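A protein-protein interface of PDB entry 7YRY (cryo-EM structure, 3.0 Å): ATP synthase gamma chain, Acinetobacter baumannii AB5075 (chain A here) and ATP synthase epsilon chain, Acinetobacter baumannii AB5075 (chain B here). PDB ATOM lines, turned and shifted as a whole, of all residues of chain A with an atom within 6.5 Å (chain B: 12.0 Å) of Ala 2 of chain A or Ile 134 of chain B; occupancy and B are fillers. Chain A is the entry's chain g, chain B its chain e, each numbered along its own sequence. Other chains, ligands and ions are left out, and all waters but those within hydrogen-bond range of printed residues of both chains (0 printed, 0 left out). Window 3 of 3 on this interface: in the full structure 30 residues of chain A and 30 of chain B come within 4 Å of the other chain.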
ATOM      1  N   ALA A   2      19.562  17.811 -13.411  1.00  0.00           N
ATOM      2  CA  ALA A   2      19.860  17.877 -11.985  1.00  0.00           C
ATOM      3  C   ALA A   2      21.347  17.655 -11.721  1.00  0.00           C
ATOM      4  O   ALA A   2      22.027  18.537 -11.196  1.00  0.00           O
ATOM      5  CB  ALA A   2      19.025  16.859 -11.221  1.00  0.00           C
ATOM      6  N   ASN A   3      21.842  16.473 -12.097  1.00  0.00           N
ATOM      7  CA  ASN A   3      23.243  16.092 -11.897  1.00  0.00           C
ATOM      8  C   ASN A   3      23.630  16.149 -10.420  1.00  0.00           C
ATOM      9  O   ASN A   3      24.671  16.697 -10.054  1.00  0.00           O
ATOM     10  CB  ASN A   3      24.177  16.963 -12.741  1.00  0.00           C
ATOM     11  CG  ASN A   3      25.501  16.288 -13.034  1.00  0.00           C
ATOM     12  OD1 ASN A   3      25.663  15.086 -12.817  1.00  0.00           O
ATOM     13  ND2 ASN A   3      26.456  17.058 -13.542  1.00  0.00           N
ATOM     14  N   LEU A   4      22.792  15.546  -9.571  1.00  0.00           N
ATOM     15  CA  LEU A   4      22.959  15.660  -8.123  1.00  0.00           C
ATOM     16  C   LEU A   4      24.296  15.090  -7.659  1.00  0.00           C
ATOM     17  O   LEU A   4      24.946  15.654  -6.764  1.00  0.00           O
ATOM     18  CB  LEU A   4      21.803  14.951  -7.418  1.00  0.00           C
ATOM     19  CG  LEU A   4      20.387  15.331  -7.863  1.00  0.00           C
ATOM     20  CD1 LEU A   4      19.499  14.096  -7.913  1.00  0.00           C
ATOM     21  CD2 LEU A   4      19.781  16.394  -6.955  1.00  0.00           C
ATOM     22  N   LYS A   5      24.716  13.968  -8.252  1.00  0.00           N
ATOM     23  CA  LYS A   5      25.969  13.333  -7.856  1.00  0.00           C
ATOM     24  C   LYS A   5      27.127  14.311  -7.984  1.00  0.00           C
ATOM     25  O   LYS A   5      27.969  14.437  -7.082  1.00  0.00           O
ATOM     26  CB  LYS A   5      26.211  12.091  -8.714  1.00  0.00           C
ATOM     27  CG  LYS A   5      24.986  11.201  -8.851  1.00  0.00           C
ATOM     28  CD  LYS A   5      24.755  10.350  -7.618  1.00  0.00           C
ATOM     29  CE  LYS A   5      23.418   9.627  -7.707  1.00  0.00           C
ATOM     30  NZ  LYS A   5      23.383   8.385  -6.889  1.00  0.00           N
ATOM     31  N   GLU A   6      27.162  15.038  -9.099  1.00  0.00           N
ATOM     32  CA  GLU A   6      28.201  16.033  -9.299  1.00  0.00           C
ATOM     33  C   GLU A   6      28.032  17.201  -8.328  1.00  0.00           C
ATOM     34  O   GLU A   6      29.014  17.859  -7.980  1.00  0.00           O
ATOM     35  CB  GLU A   6      28.213  16.455 -10.777  1.00  0.00           C
ATOM     36  CG  GLU A   6      28.994  17.716 -11.206  1.00  0.00           C
ATOM     37  CD  GLU A   6      28.493  19.010 -10.589  1.00  0.00           C
ATOM     38  OE1 GLU A   6      29.318  19.904 -10.308  1.00  0.00           O
ATOM     39  OE2 GLU A   6      27.267  19.133 -10.401  1.00  0.00           O
ATOM     40  N   ILE A   7      26.806  17.462  -7.853  1.00  0.00           N
ATOM     41  CA  ILE A   7      26.655  18.475  -6.803  1.00  0.00           C
ATOM     42  C   ILE A   7      27.347  18.047  -5.513  1.00  0.00           C
ATOM     43  O   ILE A   7      28.069  18.841  -4.896  1.00  0.00           O
ATOM     44  CB  ILE A   7      25.178  18.843  -6.550  1.00  0.00           C
ATOM     45  CG1 ILE A   7      24.601  19.691  -7.686  1.00  0.00           C
ATOM     46  CG2 ILE A   7      25.037  19.595  -5.234  1.00  0.00           C
ATOM     47  CD1 ILE A   7      23.507  19.054  -8.477  1.00  0.00           C
ATOM     48  N   ILE A 266      19.608  24.396  -3.008  1.00  0.00           N
ATOM     49  CA  ILE A 266      19.178  24.077  -4.370  1.00  0.00           C
ATOM     50  C   ILE A 266      19.108  22.564  -4.570  1.00  0.00           C
ATOM     51  O   ILE A 266      18.172  22.042  -5.197  1.00  0.00           O
ATOM     52  CB  ILE A 266      20.115  24.749  -5.390  1.00  0.00           C
ATOM     53  CG1 ILE A 266      19.806  26.242  -5.487  1.00  0.00           C
ATOM     54  CG2 ILE A 266      19.981  24.103  -6.757  1.00  0.00           C
ATOM     55  CD1 ILE A 266      20.608  26.961  -6.545  1.00  0.00           C
ATOM     56  N   LEU A 270      15.854  20.258  -5.702  1.00  0.00           N
ATOM     57  CA  LEU A 270      15.871  19.381  -6.870  1.00  0.00           C
ATOM     58  C   LEU A 270      15.573  17.935  -6.491  1.00  0.00           C
ATOM     59  O   LEU A 270      14.883  17.223  -7.231  1.00  0.00           O
ATOM     60  CB  LEU A 270      17.219  19.478  -7.585  1.00  0.00           C
ATOM     61  CG  LEU A 270      17.398  20.668  -8.528  1.00  0.00           C
ATOM     62  CD1 LEU A 270      18.833  21.157  -8.511  1.00  0.00           C
ATOM     63  CD2 LEU A 270      16.981  20.292  -9.937  1.00  0.00           C
ATOM     64  N   ALA A 274      12.546  15.676  -7.988  1.00  0.00           N
ATOM     65  CA  ALA A 274      12.794  14.419  -8.689  1.00  0.00           C
ATOM     66  C   ALA A 274      11.994  13.274  -8.083  1.00  0.00           C
ATOM     67  O   ALA A 274      11.423  12.453  -8.813  1.00  0.00           O
ATOM     68  CB  ALA A 274      14.287  14.095  -8.671  1.00  0.00           C
ATOM     69  N   GLN B 127      32.915  25.348 -12.629  1.00  0.00           N
ATOM     70  CA  GLN B 127      31.550  25.040 -13.053  1.00  0.00           C
ATOM     71  C   GLN B 127      30.605  25.235 -11.873  1.00  0.00           C
ATOM     72  O   GLN B 127      30.601  24.430 -10.935  1.00  0.00           O
ATOM     73  CB  GLN B 127      31.464  23.616 -13.609  1.00  0.00           C
ATOM     74  CG  GLN B 127      30.098  22.962 -13.508  1.00  0.00           C
ATOM     75  CD  GLN B 127      30.050  21.894 -12.435  1.00  0.00           C
ATOM     76  OE1 GLN B 127      30.944  21.053 -12.340  1.00  0.00           O
ATOM     77  NE2 GLN B 127      29.009  21.929 -11.613  1.00  0.00           N
ATOM     78  N   LEU B 128      29.829  26.322 -11.905  1.00  0.00           N
ATOM     79  CA  LEU B 128      28.800  26.584 -10.903  1.00  0.00           C
ATOM     80  C   LEU B 128      27.465  27.050 -11.472  1.00  0.00           C
ATOM     81  O   LEU B 128      26.455  26.944 -10.770  1.00  0.00           O
ATOM     82  CB  LEU B 128      29.283  27.632  -9.890  1.00  0.00           C
ATOM     83  CG  LEU B 128      29.799  27.185  -8.518  1.00  0.00           C
ATOM     84  CD1 LEU B 128      31.115  26.436  -8.609  1.00  0.00           C
ATOM     85  CD2 LEU B 128      29.932  28.387  -7.600  1.00  0.00           C
ATOM     86  N   GLU B 129      27.410  27.561 -12.706  1.00  0.00           N
ATOM     87  CA  GLU B 129      26.195  28.205 -13.197  1.00  0.00           C
ATOM     88  C   GLU B 129      25.216  27.220 -13.825  1.00  0.00           C
ATOM     89  O   GLU B 129      24.006  27.478 -13.828  1.00  0.00           O
ATOM     90  CB  GLU B 129      26.553  29.293 -14.210  1.00  0.00           C
ATOM     91  CG  GLU B 129      25.568  30.451 -14.258  1.00  0.00           C
ATOM     92  CD  GLU B 129      25.107  30.894 -12.882  1.00  0.00           C
ATOM     93  OE1 GLU B 129      25.969  31.189 -12.027  1.00  0.00           O
ATOM     94  OE2 GLU B 129      23.880  30.954 -12.658  1.00  0.00           O
ATOM     95  N   THR B 130      25.709  26.098 -14.357  1.00  0.00           N
ATOM     96  CA  THR B 130      24.819  25.117 -14.971  1.00  0.00           C
ATOM     97  C   THR B 130      23.861  24.516 -13.950  1.00  0.00           C
ATOM     98  O   THR B 130      22.848  23.916 -14.325  1.00  0.00           O
ATOM     99  CB  THR B 130      25.633  24.013 -15.644  1.00  0.00           C
ATOM    100  OG1 THR B 130      24.811  22.852 -15.821  1.00  0.00           O
ATOM    101  CG2 THR B 130      26.833  23.646 -14.792  1.00  0.00           C
ATOM    102  N   ILE B 131      24.167  24.665 -12.665  1.00  0.00           N
ATOM    103  CA  ILE B 131      23.297  24.184 -11.599  1.00  0.00           C
ATOM    104  C   ILE B 131      22.369  25.286 -11.111  1.00  0.00           C
ATOM    105  O   ILE B 131      21.192  25.041 -10.837  1.00  0.00           O
ATOM    106  CB  ILE B 131      24.167  23.635 -10.457  1.00  0.00           C
ATOM    107  CG1 ILE B 131      25.304  22.797 -11.039  1.00  0.00           C
ATOM    108  CG2 ILE B 131      23.322  22.827  -9.486  1.00  0.00           C
ATOM    109  CD1 ILE B 131      25.931  21.867 -10.059  1.00  0.00           C
ATOM    110  N   ARG B 132      22.893  26.508 -10.999  1.00  0.00           N
ATOM    111  CA  ARG B 132      22.077  27.638 -10.569  1.00  0.00           C
ATOM    112  C   ARG B 132      20.967  27.923 -11.572  1.00  0.00           C
ATOM    113  O   ARG B 132      19.853  28.294 -11.187  1.00  0.00           O
ATOM    114  CB  ARG B 132      22.958  28.872 -10.382  1.00  0.00           C
ATOM    115  CG  ARG B 132      23.366  29.146  -8.945  1.00  0.00           C
ATOM    116  CD  ARG B 132      23.864  30.571  -8.787  1.00  0.00           C
ATOM    117  NE  ARG B 132      25.284  30.679  -9.100  1.00  0.00           N
ATOM    118  CZ  ARG B 132      26.207  31.120  -8.257  1.00  0.00           C
ATOM    119  NH1 ARG B 132      25.897  31.499  -7.029  1.00  0.00           N
ATOM    120  NH2 ARG B 132      27.475  31.173  -8.655  1.00  0.00           N
ATOM    121  N   LYS B 133      21.254  27.758 -12.865  1.00  0.00           N
ATOM    122  CA  LYS B 133      20.277  28.056 -13.904  1.00  0.00           C
ATOM    123  C   LYS B 133      19.132  27.053 -13.957  1.00  0.00           C
ATOM    124  O   LYS B 133      18.151  27.300 -14.666  1.00  0.00           O
ATOM    125  CB  LYS B 133      20.974  28.108 -15.264  1.00  0.00           C
ATOM    126  CG  LYS B 133      21.770  29.378 -15.506  1.00  0.00           C
ATOM    127  CD  LYS B 133      22.548  29.294 -16.808  1.00  0.00           C
ATOM    128  CE  LYS B 133      23.003  30.666 -17.272  1.00  0.00           C
ATOM    129  NZ  LYS B 133      23.782  30.586 -18.540  1.00  0.00           N
ATOM    130  N   ILE B 134      19.225  25.939 -13.234  1.00  0.00           N
ATOM    131  CA  ILE B 134      18.241  24.869 -13.323  1.00  0.00           C
ATOM    132  C   ILE B 134      17.551  24.615 -11.980  1.00  0.00           C
ATOM    133  O   ILE B 134      16.985  23.548 -11.766  1.00  0.00           O
ATOM    134  CB  ILE B 134      18.880  23.581 -13.880  1.00  0.00           C
ATOM    135  CG1 ILE B 134      19.808  22.939 -12.848  1.00  0.00           C
ATOM    136  CG2 ILE B 134      19.642  23.874 -15.163  1.00  0.00           C
ATOM    137  CD1 ILE B 134      19.983  21.449 -13.034  1.00  0.00           C
ATOM    138  N   LYS B 135      17.576  25.599 -11.076  1.00  0.00           N
ATOM    139  CA  LYS B 135      17.011  25.396  -9.745  1.00  0.00           C
ATOM    140  C   LYS B 135      15.501  25.187  -9.796  1.00  0.00           C
ATOM    141  O   LYS B 135      14.962  24.342  -9.070  1.00  0.00           O
ATOM    142  CB  LYS B 135      17.357  26.579  -8.840  1.00  0.00           C
ATOM    143  CG  LYS B 135      17.137  27.945  -9.471  1.00  0.00           C
ATOM    144  CD  LYS B 135      17.525  29.061  -8.515  1.00  0.00           C
ATOM    145  CE  LYS B 135      16.450  29.291  -7.464  1.00  0.00           C
ATOM    146  NZ  LYS B 135      15.560  30.431  -7.822  1.00  0.00           N
ATOM    147  N   ASN B 136      14.800  25.940 -10.640  1.00  0.00           N
ATOM    148  CA  ASN B 136      13.344  25.888 -10.703  1.00  0.00           C
ATOM    149  C   ASN B 136      12.822  24.851 -11.690  1.00  0.00           C
ATOM    150  O   ASN B 136      11.607  24.783 -11.905  1.00  0.00           O
ATOM    151  CB  ASN B 136      12.782  27.268 -11.060  1.00  0.00           C
ATOM    152  CG  ASN B 136      13.517  28.395 -10.359  1.00  0.00           C
ATOM    153  OD1 ASN B 136      13.742  28.348  -9.149  1.00  0.00           O
ATOM    154  ND2 ASN B 136      13.897  29.416 -11.118  1.00  0.00           N
ATOM    155  N   ARG B 137      13.702  24.056 -12.294  1.00  0.00           N
ATOM    156  CA  ARG B 137      13.270  23.030 -13.235  1.00  0.00           C
ATOM    157  C   ARG B 137      12.401  21.983 -12.551  1.00  0.00           C
ATOM    158  O   ARG B 137      12.625  21.620 -11.392  1.00  0.00           O
ATOM    159  CB  ARG B 137      14.487  22.360 -13.872  1.00  0.00           C
ATOM    160  CG  ARG B 137      15.347  23.295 -14.696  1.00  0.00           C
ATOM    161  CD  ARG B 137      15.750  22.644 -16.008  1.00  0.00           C
ATOM    162  NE  ARG B 137      14.683  21.820 -16.561  1.00  0.00           N
ATOM    163  CZ  ARG B 137      14.883  20.743 -17.308  1.00  0.00           C
ATOM    164  NH1 ARG B 137      16.102  20.338 -17.625  1.00  0.00           N
ATOM    165  NH2 ARG B 137      13.835  20.050 -17.743  1.00  0.00           N
ATOM    166  N   ALA B 138      11.400  21.495 -13.284  1.00  0.00           N
ATOM    167  CA  ALA B 138      10.550  20.407 -12.828  1.00  0.00           C
ATOM    168  C   ALA B 138      10.672  19.155 -13.684  1.00  0.00           C
ATOM    169  O   ALA B 138      10.063  18.135 -13.346  1.00  0.00           O
ATOM    170  CB  ALA B 138       9.080  20.854 -12.794  1.00  0.00           C
ATOM    171  N   GLN B 139      11.435  19.212 -14.776  1.00  0.00           N
ATOM    172  CA  GLN B 139      11.663  18.072 -15.663  1.00  0.00           C
ATOM    173  C   GLN B 139      10.358  17.488 -16.200  1.00  0.00           C
ATOM    174  O   GLN B 139       9.834  16.511 -15.667  1.00  0.00           O
ATOM    175  CB  GLN B 139      12.469  16.987 -14.944  1.00  0.00           C
ATOM    176  CG  GLN B 139      13.960  17.023 -15.241  1.00  0.00           C
ATOM    177  CD  GLN B 139      14.715  15.886 -14.584  1.00  0.00           C
ATOM    178  OE1 GLN B 139      14.486  15.564 -13.418  1.00  0.00           O
ATOM    179  NE2 GLN B 139      15.623  15.268 -15.331  1.00  0.00           N
ATOM    180  OXT GLN B 139       9.802  17.976 -17.184  1.00  0.00           O
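OE1 of Glu 6 of chain A sits at hydrogen-bond distance from NE2 of Gln 127 of chain B (2.4 Å).
The side-chain amide oxygen (OD1) of Asn 136 of chain B is in hydrogen-bond range of the side-chain amino group (NZ) of Lys 135 of chain B, at 3.1 Å.
Ile 134 of chain B touches Ala 2 of chain A (CD1 to N, 3.7 Å).
Glu 6 of chain A touches Ile 131 of chain B.
CG1 of Ile 7 of chain A touches CD1 of Ile 131 of chain B (3.5 Å).
Lys 135 of chain B touches Ile 266 of chain A (CB to CD1, 3.998 Å).
O of Ile 134 of chain B touches CD2 of Leu 270 of chain A, 3.7 Å away.
Ala 2 of chain A touches just one residue of chain B: Ile 134 (3.7 Å).
Ile 134 of chain B touches just these residues of chain A: Ala 2 and Leu 270.
No residue of chain B comes within 4 Å of Asn 3 of chain A.
No residue of chain B comes within 4 Å of Leu 4 of chain A.
Of chain B, only Gln 127 (2.4 Å) and Ile 131 (3.1 Å) come within 4 Å of Glu 6 of chain A.
Leu 270 of chain A touches one residue of chain B.
Of the printed residues of chain B, Ile 266 of chain A touches Lys 135.
Of the printed residues of chain A, Ile 131 of chain B touches Glu 6 (3.1 Å) and Ile 7 (3.5 Å).
Lys 5 of chain A touches none of the printed residues of chain B.
The nearest printed residue of chain A that does not touch Lys 135 of chain B is Leu 270 of chain A (4.4 Å).
Hydrophobic or aromatic side chains of chain B within 4 Å of the printed part of chain A: Ile 131 and Ile 134.
Of the 9 printed residues of chain A, 5 touch a printed residue of chain B.
Hydrophobic or aromatic side chains of chain A within 4 Å of the printed part of chain B: Ile 7, Ile 266 and Leu 270.
Among the printed residues, 6 pairs touch across the chains.
Among the printed residues, no Asp or Glu carboxylate lies within 4 Å of a Lys or Arg side-chain nitrogen of the other chain.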
